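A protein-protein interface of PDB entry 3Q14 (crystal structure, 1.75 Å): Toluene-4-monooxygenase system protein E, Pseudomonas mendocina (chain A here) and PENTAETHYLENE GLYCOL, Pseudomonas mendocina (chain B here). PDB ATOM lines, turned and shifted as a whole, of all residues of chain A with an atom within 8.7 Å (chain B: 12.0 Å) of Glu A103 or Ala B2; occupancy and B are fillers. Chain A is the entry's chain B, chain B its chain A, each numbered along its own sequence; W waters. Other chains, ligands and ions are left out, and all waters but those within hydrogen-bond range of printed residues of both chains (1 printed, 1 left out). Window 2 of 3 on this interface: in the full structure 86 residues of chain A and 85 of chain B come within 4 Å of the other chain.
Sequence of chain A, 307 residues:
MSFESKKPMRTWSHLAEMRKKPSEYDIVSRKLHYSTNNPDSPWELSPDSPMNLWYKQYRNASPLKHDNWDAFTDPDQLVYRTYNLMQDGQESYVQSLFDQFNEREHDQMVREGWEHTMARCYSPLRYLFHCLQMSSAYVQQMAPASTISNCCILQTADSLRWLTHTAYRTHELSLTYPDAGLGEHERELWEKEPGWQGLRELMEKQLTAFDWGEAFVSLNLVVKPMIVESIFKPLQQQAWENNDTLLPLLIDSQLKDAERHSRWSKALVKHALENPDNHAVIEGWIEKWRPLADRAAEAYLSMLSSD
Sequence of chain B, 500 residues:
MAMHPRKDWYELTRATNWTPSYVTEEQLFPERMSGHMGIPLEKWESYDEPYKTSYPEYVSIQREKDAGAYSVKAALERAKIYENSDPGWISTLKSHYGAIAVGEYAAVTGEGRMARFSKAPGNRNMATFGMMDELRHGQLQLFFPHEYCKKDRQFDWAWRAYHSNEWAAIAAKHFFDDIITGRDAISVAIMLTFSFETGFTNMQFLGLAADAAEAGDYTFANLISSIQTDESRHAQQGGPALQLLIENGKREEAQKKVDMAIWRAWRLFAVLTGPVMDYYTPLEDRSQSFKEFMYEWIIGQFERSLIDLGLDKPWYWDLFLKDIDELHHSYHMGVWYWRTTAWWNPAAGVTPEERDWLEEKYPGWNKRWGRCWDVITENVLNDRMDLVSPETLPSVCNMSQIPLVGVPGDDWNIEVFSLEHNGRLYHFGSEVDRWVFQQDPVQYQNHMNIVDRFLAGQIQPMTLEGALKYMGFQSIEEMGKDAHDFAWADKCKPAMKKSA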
ATOM      1  N   GLN A  95      -6.810 -23.312   2.659  1.00  0.00           N
ATOM      2  CA  GLN A  95      -6.278 -22.265   3.528  1.00  0.00           C
ATOM      3  C   GLN A  95      -4.875 -22.632   4.044  1.00  0.00           C
ATOM      4  O   GLN A  95      -4.000 -21.770   4.172  1.00  0.00           O
ATOM      5  CB  GLN A  95      -7.260 -21.937   4.659  1.00  0.00           C
ATOM      6  CG  GLN A  95      -8.657 -21.453   4.160  1.00  0.00           C
ATOM      7  CD  GLN A  95      -8.642 -20.063   3.508  1.00  0.00           C
ATOM      8  OE1 GLN A  95      -8.178 -19.094   4.109  1.00  0.00           O
ATOM      9  NE2 GLN A  95      -9.168 -19.967   2.282  1.00  0.00           N
ATOM     10  N   SER A  96      -4.650 -23.920   4.302  1.00  0.00           N
ATOM     11  CA  SER A  96      -3.324 -24.419   4.677  1.00  0.00           C
ATOM     12  C   SER A  96      -2.307 -24.293   3.549  1.00  0.00           C
ATOM     13  O   SER A  96      -1.135 -23.974   3.790  1.00  0.00           O
ATOM     14  CB  SER A  96      -3.406 -25.881   5.143  1.00  0.00           C
ATOM     15  OG  SER A  96      -4.008 -25.947   6.425  1.00  0.00           O
ATOM     16  N   LEU A  97      -2.746 -24.566   2.320  1.00  0.00           N
ATOM     17  CA  LEU A  97      -1.898 -24.334   1.157  1.00  0.00           C
ATOM     18  C   LEU A  97      -1.514 -22.857   1.062  1.00  0.00           C
ATOM     19  O   LEU A  97      -0.347 -22.532   0.845  1.00  0.00           O
ATOM     20  CB  LEU A  97      -2.605 -24.748  -0.133  1.00  0.00           C
ATOM     21  CG  LEU A  97      -2.746 -26.247  -0.391  1.00  0.00           C
ATOM     22  CD1 LEU A  97      -3.622 -26.459  -1.628  1.00  0.00           C
ATOM     23  CD2 LEU A  97      -1.373 -26.895  -0.565  1.00  0.00           C
ATOM     24  N   PHE A  98      -2.499 -21.971   1.191  1.00  0.00           N
ATOM     25  CA  PHE A  98      -2.235 -20.529   1.110  1.00  0.00           C
ATOM     26  C   PHE A  98      -1.179 -20.139   2.139  1.00  0.00           C
ATOM     27  O   PHE A  98      -0.226 -19.417   1.831  1.00  0.00           O
ATOM     28  CB  PHE A  98      -3.496 -19.705   1.374  1.00  0.00           C
ATOM     29  CG  PHE A  98      -4.484 -19.704   0.234  1.00  0.00           C
ATOM     30  CD1 PHE A  98      -5.732 -19.133   0.395  1.00  0.00           C
ATOM     31  CD2 PHE A  98      -4.173 -20.293  -0.984  1.00  0.00           C
ATOM     32  CE1 PHE A  98      -6.655 -19.117  -0.650  1.00  0.00           C
ATOM     33  CE2 PHE A  98      -5.093 -20.296  -2.022  1.00  0.00           C
ATOM     34  CZ  PHE A  98      -6.329 -19.699  -1.858  1.00  0.00           C
ATOM     35  N   ASP A  99      -1.366 -20.615   3.366  1.00  0.00           N
ATOM     36  CA  ASP A  99      -0.464 -20.285   4.470  1.00  0.00           C
ATOM     37  C   ASP A  99       0.951 -20.769   4.172  1.00  0.00           C
ATOM     38  O   ASP A  99       1.908 -20.013   4.300  1.00  0.00           O
ATOM     39  CB  ASP A  99      -0.993 -20.890   5.770  1.00  0.00           C
ATOM     40  CG  ASP A  99      -0.200 -20.461   6.984  1.00  0.00           C
ATOM     41  OD1 ASP A  99       0.438 -19.392   6.937  1.00  0.00           O
ATOM     42  OD2 ASP A  99      -0.227 -21.194   7.995  1.00  0.00           O
ATOM     43  N   GLN A 100       1.078 -22.028   3.757  1.00  0.00           N
ATOM     44  CA  GLN A 100       2.386 -22.640   3.541  1.00  0.00           C
ATOM     45  C   GLN A 100       3.108 -22.035   2.340  1.00  0.00           C
ATOM     46  O   GLN A 100       4.313 -21.798   2.390  1.00  0.00           O
ATOM     47  CB  GLN A 100       2.249 -24.157   3.367  1.00  0.00           C
ATOM     48  CG  GLN A 100       3.582 -24.885   3.281  1.00  0.00           C
ATOM     49  CD  GLN A 100       4.522 -24.501   4.412  1.00  0.00           C
ATOM     50  OE1 GLN A 100       4.122 -24.435   5.578  1.00  0.00           O
ATOM     51  NE2 GLN A 100       5.774 -24.222   4.070  1.00  0.00           N
ATOM     52  N   PHE A 101       2.381 -21.793   1.255  1.00  0.00           N
ATOM     53  CA  PHE A 101       3.020 -21.238   0.070  1.00  0.00           C
ATOM     54  C   PHE A 101       3.458 -19.800   0.292  1.00  0.00           C
ATOM     55  O   PHE A 101       4.492 -19.366  -0.214  1.00  0.00           O
ATOM     56  CB  PHE A 101       2.123 -21.384  -1.153  1.00  0.00           C
ATOM     57  CG  PHE A 101       2.173 -22.757  -1.754  1.00  0.00           C
ATOM     58  CD1 PHE A 101       2.743 -22.962  -3.003  1.00  0.00           C
ATOM     59  CD2 PHE A 101       1.704 -23.858  -1.045  1.00  0.00           C
ATOM     60  CE1 PHE A 101       2.811 -24.235  -3.554  1.00  0.00           C
ATOM     61  CE2 PHE A 101       1.771 -25.140  -1.592  1.00  0.00           C
ATOM     62  CZ  PHE A 101       2.326 -25.323  -2.846  1.00  0.00           C
ATOM     63  N   ASN A 102       2.675 -19.068   1.072  1.00  0.00           N
ATOM     64  CA  ASN A 102       3.066 -17.725   1.477  1.00  0.00           C
ATOM     65  C   ASN A 102       4.337 -17.746   2.348  1.00  0.00           C
ATOM     66  O   ASN A 102       5.244 -16.930   2.154  1.00  0.00           O
ATOM     67  CB  ASN A 102       1.909 -17.035   2.206  1.00  0.00           C
ATOM     68  CG  ASN A 102       2.317 -15.716   2.820  1.00  0.00           C
ATOM     69  OD1 ASN A 102       2.181 -14.656   2.201  1.00  0.00           O
ATOM     70  ND2 ASN A 102       2.836 -15.772   4.039  1.00  0.00           N
ATOM     71  N   GLU A 103       4.409 -18.679   3.295  1.00  0.00           N
ATOM     72  CA  GLU A 103       5.616 -18.823   4.117  1.00  0.00           C
ATOM     73  C   GLU A 103       6.840 -19.058   3.244  1.00  0.00           C
ATOM     74  O   GLU A 103       7.924 -18.554   3.536  1.00  0.00           O
ATOM     75  CB  GLU A 103       5.483 -19.974   5.123  1.00  0.00           C
ATOM     76  CG  GLU A 103       4.564 -19.689   6.298  1.00  0.00           C
ATOM     77  CD  GLU A 103       5.044 -18.514   7.132  1.00  0.00           C
ATOM     78  OE1 GLU A 103       4.219 -17.634   7.464  1.00  0.00           O
ATOM     79  OE2 GLU A 103       6.253 -18.473   7.457  1.00  0.00           O
ATOM     80  N   ARG A 104       6.662 -19.835   2.179  1.00  0.00           N
ATOM     81  CA  ARG A 104       7.764 -20.188   1.288  1.00  0.00           C
ATOM     82  C   ARG A 104       8.005 -19.142   0.204  1.00  0.00           C
ATOM     83  O   ARG A 104       8.870 -19.318  -0.657  1.00  0.00           O
ATOM     84  CB  ARG A 104       7.510 -21.558   0.658  1.00  0.00           C
ATOM     85  CG  ARG A 104       7.715 -22.709   1.627  1.00  0.00           C
ATOM     86  CD  ARG A 104       9.148 -22.716   2.139  1.00  0.00           C
ATOM     87  NE  ARG A 104       9.377 -23.731   3.166  1.00  0.00           N
ATOM     88  CZ  ARG A 104      10.571 -24.022   3.671  1.00  0.00           C
ATOM     89  NH1 ARG A 104      10.694 -24.958   4.603  1.00  0.00           N
ATOM     90  NH2 ARG A 104      11.648 -23.375   3.241  1.00  0.00           N
ATOM     91  N   GLU A 105       7.244 -18.054   0.258  1.00  0.00           N
ATOM     92  CA  GLU A 105       7.383 -16.957  -0.698  1.00  0.00           C
ATOM     93  C   GLU A 105       7.211 -17.443  -2.142  1.00  0.00           C
ATOM     94  O   GLU A 105       7.957 -17.053  -3.046  1.00  0.00           O
ATOM     95  CB  GLU A 105       8.720 -16.239  -0.498  1.00  0.00           C
ATOM     96  CG  GLU A 105       8.824 -15.537   0.851  1.00  0.00           C
ATOM     97  CD  GLU A 105      10.232 -15.036   1.154  1.00  0.00           C
ATOM     98  OE1 GLU A 105      11.002 -15.776   1.804  1.00  0.00           O
ATOM     99  OE2 GLU A 105      10.569 -13.902   0.747  1.00  0.00           O
ATOM    100  N   HIS A 106       6.206 -18.289  -2.338  1.00  0.00           N
ATOM    101  CA  HIS A 106       5.893 -18.858  -3.647  1.00  0.00           C
ATOM    102  C   HIS A 106       5.779 -17.799  -4.736  1.00  0.00           C
ATOM    103  O   HIS A 106       6.283 -17.972  -5.841  1.00  0.00           O
ATOM    104  CB  HIS A 106       4.585 -19.657  -3.566  1.00  0.00           C
ATOM    105  CG  HIS A 106       3.992 -19.989  -4.904  1.00  0.00           C
ATOM    106  ND1 HIS A 106       3.181 -19.116  -5.600  1.00  0.00           N
ATOM    107  CD2 HIS A 106       4.082 -21.106  -5.667  1.00  0.00           C
ATOM    108  CE1 HIS A 106       2.805 -19.677  -6.737  1.00  0.00           C
ATOM    109  NE2 HIS A 106       3.338 -20.885  -6.801  1.00  0.00           N
ATOM    110  N   ASP A 107       5.114 -16.695  -4.421  1.00  0.00           N
ATOM    111  CA  ASP A 107       4.794 -15.701  -5.442  1.00  0.00           C
ATOM    112  C   ASP A 107       6.033 -15.003  -6.012  1.00  0.00           C
ATOM    113  O   ASP A 107       6.035 -14.583  -7.165  1.00  0.00           O
ATOM    114  CB  ASP A 107       3.789 -14.683  -4.901  1.00  0.00           C
ATOM    115  CG  ASP A 107       2.406 -15.292  -4.670  1.00  0.00           C
ATOM    116  OD1 ASP A 107       1.571 -14.632  -4.018  1.00  0.00           O
ATOM    117  OD2 ASP A 107       2.148 -16.422  -5.143  1.00  0.00           O
ATOM    118  N   GLN A 108       7.086 -14.898  -5.209  1.00  0.00           N
ATOM    119  CA  GLN A 108       8.336 -14.288  -5.669  1.00  0.00           C
ATOM    120  C   GLN A 108       9.070 -15.133  -6.707  1.00  0.00           C
ATOM    121  O   GLN A 108       9.927 -14.626  -7.429  1.00  0.00           O
ATOM    122  CB  GLN A 108       9.279 -14.027  -4.484  1.00  0.00           C
ATOM    123  CG  GLN A 108       8.782 -12.958  -3.526  1.00  0.00           C
ATOM    124  CD  GLN A 108       9.711 -12.727  -2.344  1.00  0.00           C
ATOM    125  OE1 GLN A 108      10.907 -13.020  -2.406  1.00  0.00           O
ATOM    126  NE2 GLN A 108       9.157 -12.196  -1.256  1.00  0.00           N
ATOM    127  N   MET A 109       8.718 -16.414  -6.785  1.00  0.00           N
ATOM    128  CA  MET A 109       9.482 -17.373  -7.581  1.00  0.00           C
ATOM    129  C   MET A 109       8.833 -17.736  -8.912  1.00  0.00           C
ATOM    130  O   MET A 109       9.378 -18.538  -9.671  1.00  0.00           O
ATOM    131  CB  MET A 109       9.743 -18.647  -6.770  1.00  0.00           C
ATOM    132  CG  MET A 109      10.646 -18.446  -5.565  1.00  0.00           C
ATOM    133  SD  MET A 109      10.981 -19.989  -4.691  1.00  0.00           S
ATOM    134  CE  MET A 109       9.337 -20.437  -4.134  1.00  0.00           C
ATOM    135  N   TYR A 168      -8.981 -13.435  -2.505  1.00  0.00           N
ATOM    136  CA  TYR A 168      -7.866 -13.576  -1.575  1.00  0.00           C
ATOM    137  C   TYR A 168      -6.533 -13.573  -2.316  1.00  0.00           C
ATOM    138  O   TYR A 168      -5.587 -12.892  -1.916  1.00  0.00           O
ATOM    139  CB  TYR A 168      -7.999 -14.873  -0.775  1.00  0.00           C
ATOM    140  CG  TYR A 168      -6.930 -15.013   0.288  1.00  0.00           C
ATOM    141  CD1 TYR A 168      -7.135 -14.508   1.574  1.00  0.00           C
ATOM    142  CD2 TYR A 168      -5.723 -15.622   0.006  1.00  0.00           C
ATOM    143  CE1 TYR A 168      -6.161 -14.623   2.554  1.00  0.00           C
ATOM    144  CE2 TYR A 168      -4.738 -15.747   0.986  1.00  0.00           C
ATOM    145  CZ  TYR A 168      -4.968 -15.244   2.251  1.00  0.00           C
ATOM    146  OH  TYR A 168      -3.992 -15.362   3.219  1.00  0.00           O
ATOM    147  N   GLU A 172      -3.384 -11.105  -2.289  1.00  0.00           N
ATOM    148  CA  GLU A 172      -2.085 -11.628  -1.884  1.00  0.00           C
ATOM    149  C   GLU A 172      -1.007 -11.395  -2.947  1.00  0.00           C
ATOM    150  O   GLU A 172       0.108 -10.964  -2.638  1.00  0.00           O
ATOM    151  CB  GLU A 172      -2.191 -13.109  -1.539  1.00  0.00           C
ATOM    152  CG  GLU A 172      -0.869 -13.704  -1.100  1.00  0.00           C
ATOM    153  CD  GLU A 172      -1.051 -15.046  -0.438  1.00  0.00           C
ATOM    154  OE1 GLU A 172      -0.592 -15.202   0.718  1.00  0.00           O
ATOM    155  OE2 GLU A 172      -1.666 -15.934  -1.069  1.00  0.00           O
ATOM    156  N   LEU A 175       0.541  -7.978  -3.106  1.00  0.00           N
ATOM    157  CA  LEU A 175       1.504  -7.625  -2.070  1.00  0.00           C
ATOM    158  C   LEU A 175       2.940  -7.818  -2.561  1.00  0.00           C
ATOM    159  O   LEU A 175       3.839  -7.071  -2.177  1.00  0.00           O
ATOM    160  CB  LEU A 175       1.255  -8.442  -0.802  1.00  0.00           C
ATOM    161  CG  LEU A 175      -0.098  -8.200  -0.123  1.00  0.00           C
ATOM    162  CD1 LEU A 175      -0.251  -9.101   1.094  1.00  0.00           C
ATOM    163  CD2 LEU A 175      -0.262  -6.743   0.250  1.00  0.00           C
ATOM    164  N   ALA B   2       1.974 -17.232   6.307  1.00  0.00           N
ATOM    165  CA  ALA B   2       1.056 -16.311   6.969  1.00  0.00           C
ATOM    166  C   ALA B   2      -0.253 -16.195   6.194  1.00  0.00           C
ATOM    167  O   ALA B   2      -0.310 -16.534   5.010  1.00  0.00           O
ATOM    168  CB  ALA B   2       1.696 -14.945   7.112  1.00  0.00           C
ATOM    169  N   MET B   3      -1.295 -15.726   6.882  1.00  0.00           N
ATOM    170  CA  MET B   3      -2.610 -15.492   6.286  1.00  0.00           C
ATOM    171  C   MET B   3      -2.913 -14.007   6.417  1.00  0.00           C
ATOM    172  O   MET B   3      -2.545 -13.365   7.409  1.00  0.00           O
ATOM    173  CB  MET B   3      -3.699 -16.283   7.010  1.00  0.00           C
ATOM    174  CG  MET B   3      -3.527 -17.796   6.965  1.00  0.00           C
ATOM    175  SD  MET B   3      -3.542 -18.415   5.280  1.00  0.00           S
ATOM    176  CE  MET B   3      -5.270 -18.174   4.827  1.00  0.00           C
ATOM    177  N   HIS B   4      -3.572 -13.452   5.410  1.00  0.00           N
ATOM    178  CA  HIS B   4      -3.889 -12.035   5.443  1.00  0.00           C
ATOM    179  C   HIS B   4      -5.271 -11.828   6.029  1.00  0.00           C
ATOM    180  O   HIS B   4      -6.182 -12.580   5.731  1.00  0.00           O
ATOM    181  CB  HIS B   4      -3.753 -11.460   4.036  1.00  0.00           C
ATOM    182  CG  HIS B   4      -2.427 -11.767   3.425  1.00  0.00           C
ATOM    183  ND1 HIS B   4      -2.261 -12.723   2.444  1.00  0.00           N
ATOM    184  CD2 HIS B   4      -1.186 -11.325   3.734  1.00  0.00           C
ATOM    185  CE1 HIS B   4      -0.979 -12.816   2.139  1.00  0.00           C
ATOM    186  NE2 HIS B   4      -0.305 -11.978   2.906  1.00  0.00           N
ATOM    187  N   PRO B   5      -5.416 -10.814   6.895  1.00  0.00           N
ATOM    188  CA  PRO B   5      -6.673 -10.578   7.604  1.00  0.00           C
ATOM    189  C   PRO B   5      -7.791 -10.207   6.636  1.00  0.00           C
ATOM    190  O   PRO B   5      -7.551  -9.585   5.596  1.00  0.00           O
ATOM    191  CB  PRO B   5      -6.347  -9.389   8.518  1.00  0.00           C
ATOM    192  CG  PRO B   5      -5.156  -8.742   7.900  1.00  0.00           C
ATOM    193  CD  PRO B   5      -4.373  -9.852   7.279  1.00  0.00           C
ATOM    194  N   ARG B   6      -9.007 -10.582   6.996  1.00  0.00           N
ATOM    195  CA  ARG B   6     -10.153 -10.401   6.106  1.00  0.00           C
ATOM    196  C   ARG B   6     -10.291  -8.947   5.691  1.00  0.00           C
ATOM    197  O   ARG B   6     -10.657  -8.656   4.551  1.00  0.00           O
ATOM    198  CB  ARG B   6     -11.437 -10.837   6.803  1.00  0.00           C
ATOM    199  CG  ARG B   6     -12.655 -10.828   5.890  1.00  0.00           C
ATOM    200  CD  ARG B   6     -13.865 -11.363   6.643  1.00  0.00           C
ATOM    201  NE  ARG B   6     -14.324 -10.380   7.612  1.00  0.00           N
ATOM    202  CZ  ARG B   6     -15.106 -10.644   8.655  1.00  0.00           C
ATOM    203  NH1 ARG B   6     -15.521 -11.883   8.896  1.00  0.00           N
ATOM    204  NH2 ARG B   6     -15.460  -9.659   9.469  1.00  0.00           N
ATOM    205  N   ASP B   8      -8.319  -6.815   4.842  1.00  0.00           N
ATOM    206  CA  ASP B   8      -7.442  -6.442   3.735  1.00  0.00           C
ATOM    207  C   ASP B   8      -7.918  -6.899   2.353  1.00  0.00           C
ATOM    208  O   ASP B   8      -7.535  -6.314   1.339  1.00  0.00           O
ATOM    209  CB  ASP B   8      -6.029  -6.971   3.970  1.00  0.00           C
ATOM    210  CG  ASP B   8      -5.356  -6.325   5.161  1.00  0.00           C
ATOM    211  OD1 ASP B   8      -5.894  -5.323   5.675  1.00  0.00           O
ATOM    212  OD2 ASP B   8      -4.287  -6.820   5.570  1.00  0.00           O
ATOM    213  N   TRP B   9      -8.736  -7.945   2.304  1.00  0.00           N
ATOM    214  CA  TRP B   9      -9.200  -8.462   1.015  1.00  0.00           C
ATOM    215  C   TRP B   9     -10.721  -8.492   0.874  1.00  0.00           C
ATOM    216  O   TRP B   9     -11.238  -8.821  -0.197  1.00  0.00           O
ATOM    217  CB  TRP B   9      -8.608  -9.859   0.741  1.00  0.00           C
ATOM    218  CG  TRP B   9      -8.743 -10.836   1.892  1.00  0.00           C
ATOM    219  CD1 TRP B   9      -7.805 -11.093   2.856  1.00  0.00           C
ATOM    220  CD2 TRP B   9      -9.863 -11.679   2.191  1.00  0.00           C
ATOM    221  NE1 TRP B   9      -8.276 -12.035   3.737  1.00  0.00           N
ATOM    222  CE2 TRP B   9      -9.537 -12.409   3.357  1.00  0.00           C
ATOM    223  CE3 TRP B   9     -11.118 -11.879   1.597  1.00  0.00           C
ATOM    224  CZ2 TRP B   9     -10.408 -13.335   3.931  1.00  0.00           C
ATOM    225  CZ3 TRP B   9     -11.984 -12.797   2.174  1.00  0.00           C
ATOM    226  CH2 TRP B   9     -11.626 -13.511   3.332  1.00  0.00           C
HETATM  227  O   HOH W   1      -4.670 -21.232   7.082  1.00  0.00           O
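Printed residues of chain A that touch a printed residue of chain B: Gln A95, Asp A99, Asn A102, Glu A103, Tyr A168, Glu A172 and Leu A175. Among the printed residues, 11 pairs touch across the chains. Among the printed residues, no Asp or Glu carboxylate lies within 4 Å of a Lys or Arg side-chain nitrogen of the other chain.
The backbone carbonyl oxygen (O) of Gln A95 sits close to the side-chain sulfur (SD) of Met B3 (3.6 Å). N of Asp A99 lies close to SD of Met B3, 3.6 Å away. N of His B4 sits at hydrogen-bond distance from OH of Tyr A168 (2.9 Å). The backbone NH of Ala B2 sits at hydrogen-bond distance from the side-chain carboxylate of Glu A103, at 2.6 Å. The side-chain sulfur of Met B3 sits close to the side-chain hydroxyl of Tyr A168, at 3.7 Å. The backbone NH (N) of Ala B2 sits close to the side-chain amide nitrogen (ND2) of Asn A102 (2.8 Å). The backbone NH of Ala B2 is in hydrogen-bond range of the side-chain carboxylate of Asp A99 (2.7 Å). OE1 of Glu A172 lies close to ND1 of His B4 (3.5 Å).
His B4 touches Asn A102 (CE1 to OD1, 3.7 Å). Tyr A168 touches Trp B9 (CD1 to NE1, 3.5 Å). Leu A175 touches His B4.
Water W1 bridges the backbone carbonyl oxygen (O) of Gln A95 (3.0 Å) and the side-chain sulfur (SD) of Met B3 (3.5 Å).
The side-chain amide oxygen of Asn A102 sits close to the side-chain carboxylate of Glu A172 (3.2 Å). The backbone carbonyl oxygen (O) of Pro B5 lies close to the indole nitrogen (NE1) of Trp B9. The indole nitrogen of Trp B9 lies within hydrogen-bond range of the backbone carbonyl oxygen of His B4 (2.9 Å).
Of the printed residues of chain B, Gln A95 touches Met B3 (3.1 Å). Phe A98 touches none of the printed residues of chain B. Asp A99 touches just these residues of chain B: Ala B2 (2.7 Å) and Met B3 (3.6 Å). Printed residues of chain B within 4 Å of Glu A103: Ala B2. No residue of chain B comes within 4 Å of Arg A104. Of the printed residues of chain B, Tyr A168 touches Met B3 (3.4 Å), His B4 (2.9 Å) and Trp B9 (3.5 Å). Printed residues of chain B within 4 Å of Leu A175: His B4. The nearest residue of chain B that does not touch Glu A103 is Met B3 (5.9 Å). The nearest printed residue of chain A that does not touch Trp B9 is Glu A172 (6.2 Å).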
